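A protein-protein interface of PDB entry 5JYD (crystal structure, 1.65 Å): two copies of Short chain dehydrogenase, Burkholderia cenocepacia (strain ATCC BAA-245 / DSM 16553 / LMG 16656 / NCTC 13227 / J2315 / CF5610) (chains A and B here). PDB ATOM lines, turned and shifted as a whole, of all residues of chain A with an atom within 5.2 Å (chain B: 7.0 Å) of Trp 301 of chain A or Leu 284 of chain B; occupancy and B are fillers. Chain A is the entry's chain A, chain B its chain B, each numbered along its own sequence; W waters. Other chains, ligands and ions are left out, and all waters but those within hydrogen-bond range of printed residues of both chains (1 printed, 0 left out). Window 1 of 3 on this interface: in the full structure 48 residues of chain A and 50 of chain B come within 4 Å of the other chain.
NE2 of Gln 299 of chain A lies within hydrogen-bond range of OXT of Phe 310 of chain B (2.9 Å). The backbone NH of Val 300 of chain A is in hydrogen-bond range of the chain-end carboxylate of Phe 310 of chain B. NE1 of Trp 301 of chain A lies within hydrogen-bond range of O of Gly 302 of chain B (2.9 Å). NE1 of Trp 301 of chain B lies within hydrogen-bond range of O of Gly 302 of chain A, 2.9 Å away. The chain-end carboxylate of Phe 310 of chain A sits at hydrogen-bond distance from the side-chain amide nitrogen of Gln 299 of chain B, 3.0 Å away. The backbone NH (N) of Val 300 of chain B lies within hydrogen-bond range of the chain-end carboxylate (OXT) of Phe 310 of chain A, 3.1 Å away.
Of the printed residues of chain B, Trp 301 of chain A touches Leu 284 (3.5 Å), Trp 301 (3.7 Å) and Gly 302 (2.9 Å). Of chain A, only Thr 293 and Trp 301 come within 4 Å of Leu 284 of chain B. Of the printed residues of chain B, Phe 310 of chain A touches Gln 299 and Val 300. Of the printed residues of chain B, Ala 303 of chain A touches Gln 299 (3.3 Å). Of the printed residues of chain A, Gly 302 of chain B touches Gln 299 (3.3 Å) and Trp 301 (2.9 Å). Of the printed residues of chain B, Gly 302 of chain A touches Gln 299 and Trp 301. Ile 281 of chain B touches none of the printed residues of chain A. Ala 296 of chain A touches none of the printed residues of chain B. The nearest printed residue of chain A that does not touch Gly 302 of chain B is Ala 296 of chain A (4.5 Å).
Leu 284 of chain A touches Trp 301 of chain B, and with the chains exchanged Trp 301 of chain A touches Leu 284 of chain B. Gln 299 of chain A touches Gly 302 of chain B, and with the chains exchanged Gly 302 of chain A touches Gln 299 of chain B. Gln 299 of chain A touches Ala 303 of chain B, and with the chains exchanged Ala 303 of chain A touches Gln 299 of chain B. Val 300 of chain A touches Phe 310 of chain B, and with the chains exchanged Phe 310 of chain A touches Val 300 of chain B.
Water W1 lies within hydrogen-bond range of O of Glu 280 of chain B (2.7 Å) and N of Ala 296 of chain A (3.1 Å).
N of Ala 242 of chain A is in hydrogen-bond range of O of Gln 299 of chain A (2.8 Å). The backbone carbonyl oxygen of Ala 244 of chain A sits at hydrogen-bond distance from the backbone NH of Ala 303 of chain A. The backbone carbonyl oxygen (O) of Ala 287 of chain A sits at hydrogen-bond distance from the side-chain hydroxyl (OG1) of Thr 293 of chain A (2.7 Å). O of Ala 242 of chain B sits at hydrogen-bond distance from N of Trp 301 of chain B (2.9 Å). The backbone carbonyl oxygen (O) of Trp 301 of chain B sits at hydrogen-bond distance from the backbone NH (N) of Ala 244 of chain B (2.9 Å). The backbone carbonyl oxygen (O) of Ala 303 of chain B sits at hydrogen-bond distance from the side-chain hydroxyl (OH) of Tyr 248 of chain B, 3.0 Å away.
Hydrophobic or aromatic side chains of chain A that line the printed part of chain B: Leu 284 and Trp 301. Of the 23 printed residues of chain B, 8 touch a printed residue of chain A. Among the printed residues, 15 pairs touch across the chains. Among the printed residues, no Asp or Glu carboxylate lies within 4 Å of a Lys or Arg side-chain nitrogen of the other chain.
CG of Leu 284 of chain A touches CZ2 of Trp 301 of chain B (3.6 Å). Thr 293 of chain A touches Pro 283 of chain B. Thr 293 of chain A touches Leu 284 of chain B (CG2 to CD1, 3.97 Å). O of Gly 302 of chain B touches CD of Gln 299 of chain A, 3.3 Å away. Gln 299 of chain A touches Ala 303 of chain B. CZ2 of Trp 301 of chain A touches CG of Leu 284 of chain B, 3.5 Å away. Trp 301 of chain A touches Trp 301 of chain B (CB to NE1, 3.7 Å). Gly 302 of chain A touches Gln 299 of chain B. Ala 303 of chain A touches Gln 299 of chain B (CA to OE1, 3.3 Å).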
ATOM      1  N   ALA A 242      19.618  14.906  38.913  1.00  0.00           N
ATOM      2  CA  ALA A 242      20.643  14.969  39.949  1.00  0.00           C
ATOM      3  C   ALA A 242      21.904  15.672  39.455  1.00  0.00           C
ATOM      4  O   ALA A 242      22.224  15.672  38.265  1.00  0.00           O
ATOM      5  CB  ALA A 242      20.993  13.580  40.459  1.00  0.00           C
ATOM      6  N   VAL A 243      22.616  16.273  40.402  1.00  0.00           N
ATOM      7  CA  VAL A 243      23.892  16.945  40.167  1.00  0.00           C
ATOM      8  C   VAL A 243      24.949  16.203  40.981  1.00  0.00           C
ATOM      9  O   VAL A 243      24.742  15.956  42.176  1.00  0.00           O
ATOM     10  CB  VAL A 243      23.814  18.439  40.551  1.00  0.00           C
ATOM     11  CG1 VAL A 243      25.220  19.053  40.521  1.00  0.00           C
ATOM     12  CG2 VAL A 243      22.895  19.211  39.597  1.00  0.00           C
ATOM     13  N   ALA A 244      26.088  15.867  40.339  1.00  0.00           N
ATOM     14  CA  ALA A 244      27.174  15.080  40.934  1.00  0.00           C
ATOM     15  C   ALA A 244      28.461  15.909  41.010  1.00  0.00           C
ATOM     16  O   ALA A 244      29.291  15.879  40.086  1.00  0.00           O
ATOM     17  CB  ALA A 244      27.401  13.792  40.154  1.00  0.00           C
ATOM     18  N   LEU A 284      24.654  24.547  36.795  1.00  0.00           N
ATOM     19  CA  LEU A 284      23.986  23.263  36.543  1.00  0.00           C
ATOM     20  C   LEU A 284      22.564  23.259  37.095  1.00  0.00           C
ATOM     21  O   LEU A 284      21.645  22.734  36.458  1.00  0.00           O
ATOM     22  CB  LEU A 284      24.776  22.095  37.154  1.00  0.00           C
ATOM     23  CG  LEU A 284      25.969  21.614  36.339  1.00  0.00           C
ATOM     24  CD1 LEU A 284      27.090  22.655  36.272  1.00  0.00           C
ATOM     25  CD2 LEU A 284      26.475  20.282  36.939  1.00  0.00           C
ATOM     26  N   ALA A 287      20.357  25.517  34.889  1.00  0.00           N
ATOM     27  CA  ALA A 287      20.045  24.879  33.604  1.00  0.00           C
ATOM     28  C   ALA A 287      19.023  23.757  33.770  1.00  0.00           C
ATOM     29  O   ALA A 287      18.103  23.623  32.954  1.00  0.00           O
ATOM     30  CB  ALA A 287      21.327  24.359  32.920  1.00  0.00           C
ATOM     31  N   LEU A 288      19.167  22.921  34.804  1.00  0.00           N
ATOM     32  CA  LEU A 288      18.229  21.808  34.940  1.00  0.00           C
ATOM     33  C   LEU A 288      16.817  22.292  35.234  1.00  0.00           C
ATOM     34  O   LEU A 288      15.845  21.700  34.744  1.00  0.00           O
ATOM     35  CB  LEU A 288      18.705  20.835  36.028  1.00  0.00           C
ATOM     36  CG  LEU A 288      19.884  19.945  35.616  1.00  0.00           C
ATOM     37  CD1 LEU A 288      20.450  19.295  36.885  1.00  0.00           C
ATOM     38  CD2 LEU A 288      19.456  18.862  34.651  1.00  0.00           C
ATOM     39  N   THR A 293      14.832  23.396  29.215  1.00  0.00           N
ATOM     40  CA  THR A 293      15.629  22.165  29.280  1.00  0.00           C
ATOM     41  C   THR A 293      14.705  20.957  29.445  1.00  0.00           C
ATOM     42  O   THR A 293      14.811  20.147  30.373  1.00  0.00           O
ATOM     43  CB  THR A 293      16.653  22.276  30.407  1.00  0.00           C
ATOM     44  OG1 THR A 293      17.224  23.593  30.380  1.00  0.00           O
ATOM     45  CG2 THR A 293      17.757  21.246  30.221  1.00  0.00           C
ATOM     46  N   ALA A 296      15.588  16.943  29.628  1.00  0.00           N
ATOM     47  CA  ALA A 296      16.484  16.453  30.679  1.00  0.00           C
ATOM     48  C   ALA A 296      15.621  15.928  31.826  1.00  0.00           C
ATOM     49  O   ALA A 296      14.993  16.711  32.530  1.00  0.00           O
ATOM     50  CB  ALA A 296      17.415  17.559  31.164  1.00  0.00           C
ATOM     51  N   GLN A 299      18.422  12.517  34.743  1.00  0.00           N
ATOM     52  CA  GLN A 299      19.844  12.657  34.428  1.00  0.00           C
ATOM     53  C   GLN A 299      20.684  12.874  35.686  1.00  0.00           C
ATOM     54  O   GLN A 299      20.200  13.282  36.746  1.00  0.00           O
ATOM     55  CB  GLN A 299      20.127  13.839  33.492  1.00  0.00           C
ATOM     56  CG  GLN A 299      19.058  14.156  32.426  1.00  0.00           C
ATOM     57  CD  GLN A 299      18.820  13.097  31.374  1.00  0.00           C
ATOM     58  OE1 GLN A 299      17.892  13.239  30.571  1.00  0.00           O
ATOM     59  NE2 GLN A 299      19.645  12.038  31.339  1.00  0.00           N
ATOM     60  N   VAL A 300      21.972  12.574  35.549  1.00  0.00           N
ATOM     61  CA  VAL A 300      22.980  12.895  36.560  1.00  0.00           C
ATOM     62  C   VAL A 300      24.036  13.722  35.838  1.00  0.00           C
ATOM     63  O   VAL A 300      24.796  13.188  35.032  1.00  0.00           O
ATOM     64  CB  VAL A 300      23.631  11.643  37.185  1.00  0.00           C
ATOM     65  CG1 VAL A 300      24.593  12.062  38.355  1.00  0.00           C
ATOM     66  CG2 VAL A 300      22.614  10.642  37.630  1.00  0.00           C
ATOM     67  N   TRP A 301      24.075  15.026  36.112  1.00  0.00           N
ATOM     68  CA  TRP A 301      25.057  15.904  35.487  1.00  0.00           C
ATOM     69  C   TRP A 301      26.208  16.150  36.447  1.00  0.00           C
ATOM     70  O   TRP A 301      26.019  16.756  37.509  1.00  0.00           O
ATOM     71  CB  TRP A 301      24.436  17.235  35.075  1.00  0.00           C
ATOM     72  CG  TRP A 301      23.482  17.158  33.882  1.00  0.00           C
ATOM     73  CD1 TRP A 301      23.097  16.049  33.181  1.00  0.00           C
ATOM     74  CD2 TRP A 301      22.836  18.276  33.261  1.00  0.00           C
ATOM     75  NE1 TRP A 301      22.241  16.420  32.164  1.00  0.00           N
ATOM     76  CE2 TRP A 301      22.069  17.779  32.193  1.00  0.00           C
ATOM     77  CE3 TRP A 301      22.838  19.657  33.511  1.00  0.00           C
ATOM     78  CZ2 TRP A 301      21.281  18.611  31.375  1.00  0.00           C
ATOM     79  CZ3 TRP A 301      22.088  20.493  32.681  1.00  0.00           C
ATOM     80  CH2 TRP A 301      21.305  19.955  31.626  1.00  0.00           C
ATOM     81  N   GLY A 302      27.404  15.754  36.031  1.00  0.00           N
ATOM     82  CA  GLY A 302      28.605  15.944  36.849  1.00  0.00           C
ATOM     83  C   GLY A 302      29.252  17.309  36.684  1.00  0.00           C
ATOM     84  O   GLY A 302      29.166  17.942  35.625  1.00  0.00           O
ATOM     85  N   ALA A 303      29.968  17.734  37.736  1.00  0.00           N
ATOM     86  CA  ALA A 303      30.915  18.848  37.620  1.00  0.00           C
ATOM     87  C   ALA A 303      32.047  18.518  38.587  1.00  0.00           C
ATOM     88  O   ALA A 303      31.990  18.858  39.776  1.00  0.00           O
ATOM     89  CB  ALA A 303      30.292  20.202  37.930  1.00  0.00           C
ATOM     90  N   PHE A 310      30.626  11.646  36.087  1.00  0.00           N
ATOM     91  CA  PHE A 310      29.256  11.810  35.592  1.00  0.00           C
ATOM     92  C   PHE A 310      29.141  12.969  34.601  1.00  0.00           C
ATOM     93  O   PHE A 310      28.034  13.517  34.384  1.00  0.00           O
ATOM     94  CB  PHE A 310      28.265  12.025  36.743  1.00  0.00           C
ATOM     95  CG  PHE A 310      28.100  10.819  37.631  1.00  0.00           C
ATOM     96  CD1 PHE A 310      27.355   9.735  37.203  1.00  0.00           C
ATOM     97  CD2 PHE A 310      28.645  10.778  38.904  1.00  0.00           C
ATOM     98  CE1 PHE A 310      27.166   8.616  38.010  1.00  0.00           C
ATOM     99  CE2 PHE A 310      28.448   9.660  39.726  1.00  0.00           C
ATOM    100  CZ  PHE A 310      27.706   8.593  39.282  1.00  0.00           C
ATOM    101  OXT PHE A 310      30.176  13.291  34.018  1.00  0.00           O
ATOM    102  N   PHE B  85      24.041  29.122  19.789  1.00  0.00           N
ATOM    103  CA  PHE B  85      25.330  29.793  19.905  1.00  0.00           C
ATOM    104  C   PHE B  85      25.266  31.187  19.278  1.00  0.00           C
ATOM    105  O   PHE B  85      25.746  32.173  19.853  1.00  0.00           O
ATOM    106  CB  PHE B  85      26.428  28.964  19.225  1.00  0.00           C
ATOM    107  CG  PHE B  85      26.908  27.749  20.009  1.00  0.00           C
ATOM    108  CD1 PHE B  85      26.516  27.502  21.298  1.00  0.00           C
ATOM    109  CD2 PHE B  85      27.789  26.859  19.417  1.00  0.00           C
ATOM    110  CE1 PHE B  85      26.974  26.386  21.986  1.00  0.00           C
ATOM    111  CE2 PHE B  85      28.265  25.756  20.113  1.00  0.00           C
ATOM    112  CZ  PHE B  85      27.849  25.527  21.402  1.00  0.00           C
ATOM    113  N   ILE B 198      33.180  20.099  22.842  1.00  0.00           N
ATOM    114  CA  ILE B 198      31.973  19.363  23.212  1.00  0.00           C
ATOM    115  C   ILE B 198      31.764  18.298  22.150  1.00  0.00           C
ATOM    116  O   ILE B 198      31.671  18.615  20.958  1.00  0.00           O
ATOM    117  CB  ILE B 198      30.725  20.258  23.313  1.00  0.00           C
ATOM    118  CG1 ILE B 198      30.977  21.408  24.291  1.00  0.00           C
ATOM    119  CG2 ILE B 198      29.487  19.427  23.752  1.00  0.00           C
ATOM    120  CD1 ILE B 198      29.871  22.462  24.310  1.00  0.00           C
ATOM    121  N   ALA B 242      31.055  15.984  26.929  1.00  0.00           N
ATOM    122  CA  ALA B 242      30.199  15.278  25.985  1.00  0.00           C
ATOM    123  C   ALA B 242      28.741  15.464  26.361  1.00  0.00           C
ATOM    124  O   ALA B 242      28.404  15.650  27.535  1.00  0.00           O
ATOM    125  CB  ALA B 242      30.553  13.789  25.919  1.00  0.00           C
ATOM    126  N   VAL B 243      27.883  15.432  25.339  1.00  0.00           N
ATOM    127  CA  VAL B 243      26.433  15.454  25.503  1.00  0.00           C
ATOM    128  C   VAL B 243      25.889  14.128  25.003  1.00  0.00           C
ATOM    129  O   VAL B 243      26.282  13.668  23.928  1.00  0.00           O
ATOM    130  CB  VAL B 243      25.817  16.625  24.727  1.00  0.00           C
ATOM    131  CG1 VAL B 243      24.279  16.510  24.689  1.00  0.00           C
ATOM    132  CG2 VAL B 243      26.212  17.919  25.356  1.00  0.00           C
ATOM    133  N   ALA B 244      24.965  13.530  25.772  1.00  0.00           N
ATOM    134  CA  ALA B 244      24.406  12.205  25.490  1.00  0.00           C
ATOM    135  C   ALA B 244      22.899  12.284  25.267  1.00  0.00           C
ATOM    136  O   ALA B 244      22.113  12.012  26.181  1.00  0.00           O
ATOM    137  CB  ALA B 244      24.694  11.223  26.622  1.00  0.00           C
ATOM    138  N   PRO B 245      22.459  12.590  24.046  1.00  0.00           N
ATOM    139  CA  PRO B 245      21.028  12.552  23.755  1.00  0.00           C
ATOM    140  C   PRO B 245      20.460  11.136  23.818  1.00  0.00           C
ATOM    141  O   PRO B 245      21.122  10.146  23.469  1.00  0.00           O
ATOM    142  CB  PRO B 245      20.938  13.108  22.328  1.00  0.00           C
ATOM    143  CG  PRO B 245      22.407  13.381  21.893  1.00  0.00           C
ATOM    144  CD  PRO B 245      23.285  12.713  22.835  1.00  0.00           C
ATOM    145  N   TYR B 248      15.947  11.686  19.471  1.00  0.00           N
ATOM    146  CA  TYR B 248      15.494  12.983  18.954  1.00  0.00           C
ATOM    147  C   TYR B 248      15.036  12.862  17.503  1.00  0.00           C
ATOM    148  O   TYR B 248      15.546  12.039  16.739  1.00  0.00           O
ATOM    149  CB  TYR B 248      16.594  14.053  19.025  1.00  0.00           C
ATOM    150  CG  TYR B 248      16.798  14.581  20.432  1.00  0.00           C
ATOM    151  CD1 TYR B 248      17.444  13.803  21.385  1.00  0.00           C
ATOM    152  CD2 TYR B 248      16.342  15.839  20.800  1.00  0.00           C
ATOM    153  CE1 TYR B 248      17.616  14.258  22.686  1.00  0.00           C
ATOM    154  CE2 TYR B 248      16.507  16.314  22.092  1.00  0.00           C
ATOM    155  CZ  TYR B 248      17.166  15.527  23.026  1.00  0.00           C
ATOM    156  OH  TYR B 248      17.340  15.947  24.322  1.00  0.00           O
ATOM    157  N   GLU B 280      15.313  21.218  22.261  1.00  0.00           N
ATOM    158  CA  GLU B 280      15.328  20.949  23.699  1.00  0.00           C
ATOM    159  C   GLU B 280      16.719  20.693  24.250  1.00  0.00           C
ATOM    160  O   GLU B 280      16.924  20.865  25.461  1.00  0.00           O
ATOM    161  CB  GLU B 280      14.461  19.737  24.047  1.00  0.00           C
ATOM    162  CG  GLU B 280      13.011  19.873  23.653  1.00  0.00           C
ATOM    163  CD  GLU B 280      12.159  18.682  24.049  1.00  0.00           C
ATOM    164  OE1 GLU B 280      11.562  18.710  25.143  1.00  0.00           O
ATOM    165  OE2 GLU B 280      12.055  17.735  23.241  1.00  0.00           O
ATOM    166  N   ILE B 281      17.671  20.290  23.406  1.00  0.00           N
ATOM    167  CA  ILE B 281      18.997  19.935  23.883  1.00  0.00           C
ATOM    168  C   ILE B 281      20.009  21.063  23.706  1.00  0.00           C
ATOM    169  O   ILE B 281      21.082  21.014  24.329  1.00  0.00           O
ATOM    170  CB  ILE B 281      19.482  18.630  23.201  1.00  0.00           C
ATOM    171  CG1 ILE B 281      20.557  17.946  24.052  1.00  0.00           C
ATOM    172  CG2 ILE B 281      19.999  18.896  21.802  1.00  0.00           C
ATOM    173  CD1 ILE B 281      20.880  16.527  23.594  1.00  0.00           C
ATOM    174  N   ALA B 282      19.692  22.096  22.926  1.00  0.00           N
ATOM    175  CA  ALA B 282      20.626  23.207  22.760  1.00  0.00           C
ATOM    176  C   ALA B 282      21.069  23.787  24.092  1.00  0.00           C
ATOM    177  O   ALA B 282      22.258  24.128  24.220  1.00  0.00           O
ATOM    178  CB  ALA B 282      20.011  24.312  21.887  1.00  0.00           C
ATOM    179  N   PRO B 283      20.214  23.907  25.108  1.00  0.00           N
ATOM    180  CA  PRO B 283      20.682  24.512  26.366  1.00  0.00           C
ATOM    181  C   PRO B 283      21.857  23.789  26.967  1.00  0.00           C
ATOM    182  O   PRO B 283      22.631  24.405  27.716  1.00  0.00           O
ATOM    183  CB  PRO B 283      19.435  24.449  27.268  1.00  0.00           C
ATOM    184  CG  PRO B 283      18.283  24.478  26.284  1.00  0.00           C
ATOM    185  CD  PRO B 283      18.763  23.628  25.149  1.00  0.00           C
ATOM    186  N   LEU B 284      22.004  22.486  26.713  1.00  0.00           N
ATOM    187  CA  LEU B 284      23.151  21.774  27.272  1.00  0.00           C
ATOM    188  C   LEU B 284      24.457  22.261  26.646  1.00  0.00           C
ATOM    189  O   LEU B 284      25.476  22.334  27.330  1.00  0.00           O
ATOM    190  CB  LEU B 284      23.048  20.264  27.075  1.00  0.00           C
ATOM    191  CG  LEU B 284      22.218  19.465  28.079  1.00  0.00           C
ATOM    192  CD1 LEU B 284      20.761  19.914  27.996  1.00  0.00           C
ATOM    193  CD2 LEU B 284      22.344  17.938  27.856  1.00  0.00           C
ATOM    194  N   TYR B 285      24.458  22.521  25.336  1.00  0.00           N
ATOM    195  CA  TYR B 285      25.673  22.982  24.655  1.00  0.00           C
ATOM    196  C   TYR B 285      26.063  24.370  25.125  1.00  0.00           C
ATOM    197  O   TYR B 285      27.245  24.644  25.357  1.00  0.00           O
ATOM    198  CB  TYR B 285      25.497  22.938  23.124  1.00  0.00           C
ATOM    199  CG  TYR B 285      25.389  21.492  22.613  1.00  0.00           C
ATOM    200  CD1 TYR B 285      24.203  20.766  22.750  1.00  0.00           C
ATOM    201  CD2 TYR B 285      26.479  20.838  22.026  1.00  0.00           C
ATOM    202  CE1 TYR B 285      24.103  19.436  22.306  1.00  0.00           C
ATOM    203  CE2 TYR B 285      26.367  19.491  21.595  1.00  0.00           C
ATOM    204  CZ  TYR B 285      25.187  18.817  21.733  1.00  0.00           C
ATOM    205  OH  TYR B 285      25.084  17.500  21.308  1.00  0.00           O
ATOM    206  N   VAL B 286      25.083  25.259  25.295  1.00  0.00           N
ATOM    207  CA  VAL B 286      25.369  26.597  25.795  1.00  0.00           C
ATOM    208  C   VAL B 286      25.926  26.523  27.215  1.00  0.00           C
ATOM    209  O   VAL B 286      26.942  27.150  27.529  1.00  0.00           O
ATOM    210  CB  VAL B 286      24.107  27.478  25.724  1.00  0.00           C
ATOM    211  CG1 VAL B 286      24.347  28.868  26.331  1.00  0.00           C
ATOM    212  CG2 VAL B 286      23.638  27.644  24.296  1.00  0.00           C
ATOM    213  N   ALA B 287      25.291  25.733  28.085  1.00  0.00           N
ATOM    214  CA  ALA B 287      25.742  25.669  29.474  1.00  0.00           C
ATOM    215  C   ALA B 287      27.168  25.122  29.578  1.00  0.00           C
ATOM    216  O   ALA B 287      27.979  25.631  30.362  1.00  0.00           O
ATOM    217  CB  ALA B 287      24.773  24.829  30.316  1.00  0.00           C
ATOM    218  N   LEU B 288      27.483  24.067  28.821  1.00  0.00           N
ATOM    219  CA  LEU B 288      28.830  23.502  28.865  1.00  0.00           C
ATOM    220  C   LEU B 288      29.879  24.517  28.408  1.00  0.00           C
ATOM    221  O   LEU B 288      30.962  24.611  28.999  1.00  0.00           O
ATOM    222  CB  LEU B 288      28.906  22.220  28.021  1.00  0.00           C
ATOM    223  CG  LEU B 288      28.282  21.005  28.703  1.00  0.00           C
ATOM    224  CD1 LEU B 288      28.142  19.842  27.729  1.00  0.00           C
ATOM    225  CD2 LEU B 288      29.118  20.549  29.926  1.00  0.00           C
ATOM    226  N   ALA B 289      29.578  25.301  27.371  1.00  0.00           N
ATOM    227  CA  ALA B 289      30.579  26.190  26.800  1.00  0.00           C
ATOM    228  C   ALA B 289      30.766  27.465  27.617  1.00  0.00           C
ATOM    229  O   ALA B 289      31.848  28.056  27.587  1.00  0.00           O
ATOM    230  CB  ALA B 289      30.190  26.549  25.372  1.00  0.00           C
ATOM    231  N   GLN B 299      32.897  15.623  31.511  1.00  0.00           N
ATOM    232  CA  GLN B 299      31.562  15.160  31.890  1.00  0.00           C
ATOM    233  C   GLN B 299      30.807  14.616  30.671  1.00  0.00           C
ATOM    234  O   GLN B 299      31.120  14.909  29.521  1.00  0.00           O
ATOM    235  CB  GLN B 299      30.706  16.256  32.540  1.00  0.00           C
ATOM    236  CG  GLN B 299      31.417  17.304  33.380  1.00  0.00           C
ATOM    237  CD  GLN B 299      32.103  16.808  34.632  1.00  0.00           C
ATOM    238  OE1 GLN B 299      32.826  17.583  35.302  1.00  0.00           O
ATOM    239  NE2 GLN B 299      31.858  15.555  35.008  1.00  0.00           N
ATOM    240  N   VAL B 300      29.780  13.834  30.966  1.00  0.00           N
ATOM    241  CA  VAL B 300      28.798  13.352  29.986  1.00  0.00           C
ATOM    242  C   VAL B 300      27.427  13.781  30.503  1.00  0.00           C
ATOM    243  O   VAL B 300      26.908  13.190  31.468  1.00  0.00           O
ATOM    244  CB  VAL B 300      28.832  11.832  29.795  1.00  0.00           C
ATOM    245  CG1 VAL B 300      27.842  11.442  28.679  1.00  0.00           C
ATOM    246  CG2 VAL B 300      30.181  11.333  29.464  1.00  0.00           C
ATOM    247  N   TRP B 301      26.822  14.773  29.862  1.00  0.00           N
ATOM    248  CA  TRP B 301      25.524  15.276  30.298  1.00  0.00           C
ATOM    249  C   TRP B 301      24.432  14.713  29.394  1.00  0.00           C
ATOM    250  O   TRP B 301      24.414  14.987  28.178  1.00  0.00           O
ATOM    251  CB  TRP B 301      25.478  16.804  30.302  1.00  0.00           C
ATOM    252  CG  TRP B 301      26.261  17.465  31.415  1.00  0.00           C
ATOM    253  CD1 TRP B 301      27.062  16.862  32.366  1.00  0.00           C
ATOM    254  CD2 TRP B 301      26.288  18.859  31.690  1.00  0.00           C
ATOM    255  NE1 TRP B 301      27.588  17.827  33.210  1.00  0.00           N
ATOM    256  CE2 TRP B 301      27.129  19.058  32.809  1.00  0.00           C
ATOM    257  CE3 TRP B 301      25.708  19.969  31.079  1.00  0.00           C
ATOM    258  CZ2 TRP B 301      27.401  20.321  33.310  1.00  0.00           C
ATOM    259  CZ3 TRP B 301      25.966  21.224  31.592  1.00  0.00           C
ATOM    260  CH2 TRP B 301      26.780  21.393  32.699  1.00  0.00           C
ATOM    261  N   GLY B 302      23.537  13.919  29.985  1.00  0.00           N
ATOM    262  CA  GLY B 302      22.463  13.325  29.225  1.00  0.00           C
ATOM    263  C   GLY B 302      21.229  14.222  29.097  1.00  0.00           C
ATOM    264  O   GLY B 302      20.943  15.110  29.921  1.00  0.00           O
ATOM    265  N   ALA B 303      20.463  13.981  28.024  1.00  0.00           N
ATOM    266  CA  ALA B 303      19.120  14.549  27.885  1.00  0.00           C
ATOM    267  C   ALA B 303      18.294  13.513  27.115  1.00  0.00           C
ATOM    268  O   ALA B 303      18.217  13.572  25.889  1.00  0.00           O
ATOM    269  CB  ALA B 303      19.106  15.903  27.174  1.00  0.00           C
ATOM    270  N   PHE B 310      22.539   8.971  31.253  1.00  0.00           N
ATOM    271  CA  PHE B 310      23.659   9.848  31.601  1.00  0.00           C
ATOM    272  C   PHE B 310      23.159  11.132  32.243  1.00  0.00           C
ATOM    273  O   PHE B 310      23.889  12.148  32.233  1.00  0.00           O
ATOM    274  CB  PHE B 310      24.529  10.184  30.373  1.00  0.00           C
ATOM    275  CG  PHE B 310      25.348   9.002  29.845  1.00  0.00           C
ATOM    276  CD1 PHE B 310      26.470   8.531  30.528  1.00  0.00           C
ATOM    277  CD2 PHE B 310      25.023   8.408  28.624  1.00  0.00           C
ATOM    278  CE1 PHE B 310      27.220   7.455  30.010  1.00  0.00           C
ATOM    279  CE2 PHE B 310      25.763   7.348  28.131  1.00  0.00           C
ATOM    280  CZ  PHE B 310      26.851   6.874  28.806  1.00  0.00           C
ATOM    281  OXT PHE B 310      22.038  11.157  32.779  1.00  0.00           O
HETATM  282  O   HOH W   1      16.506  19.051  27.479  1.00  0.00           O
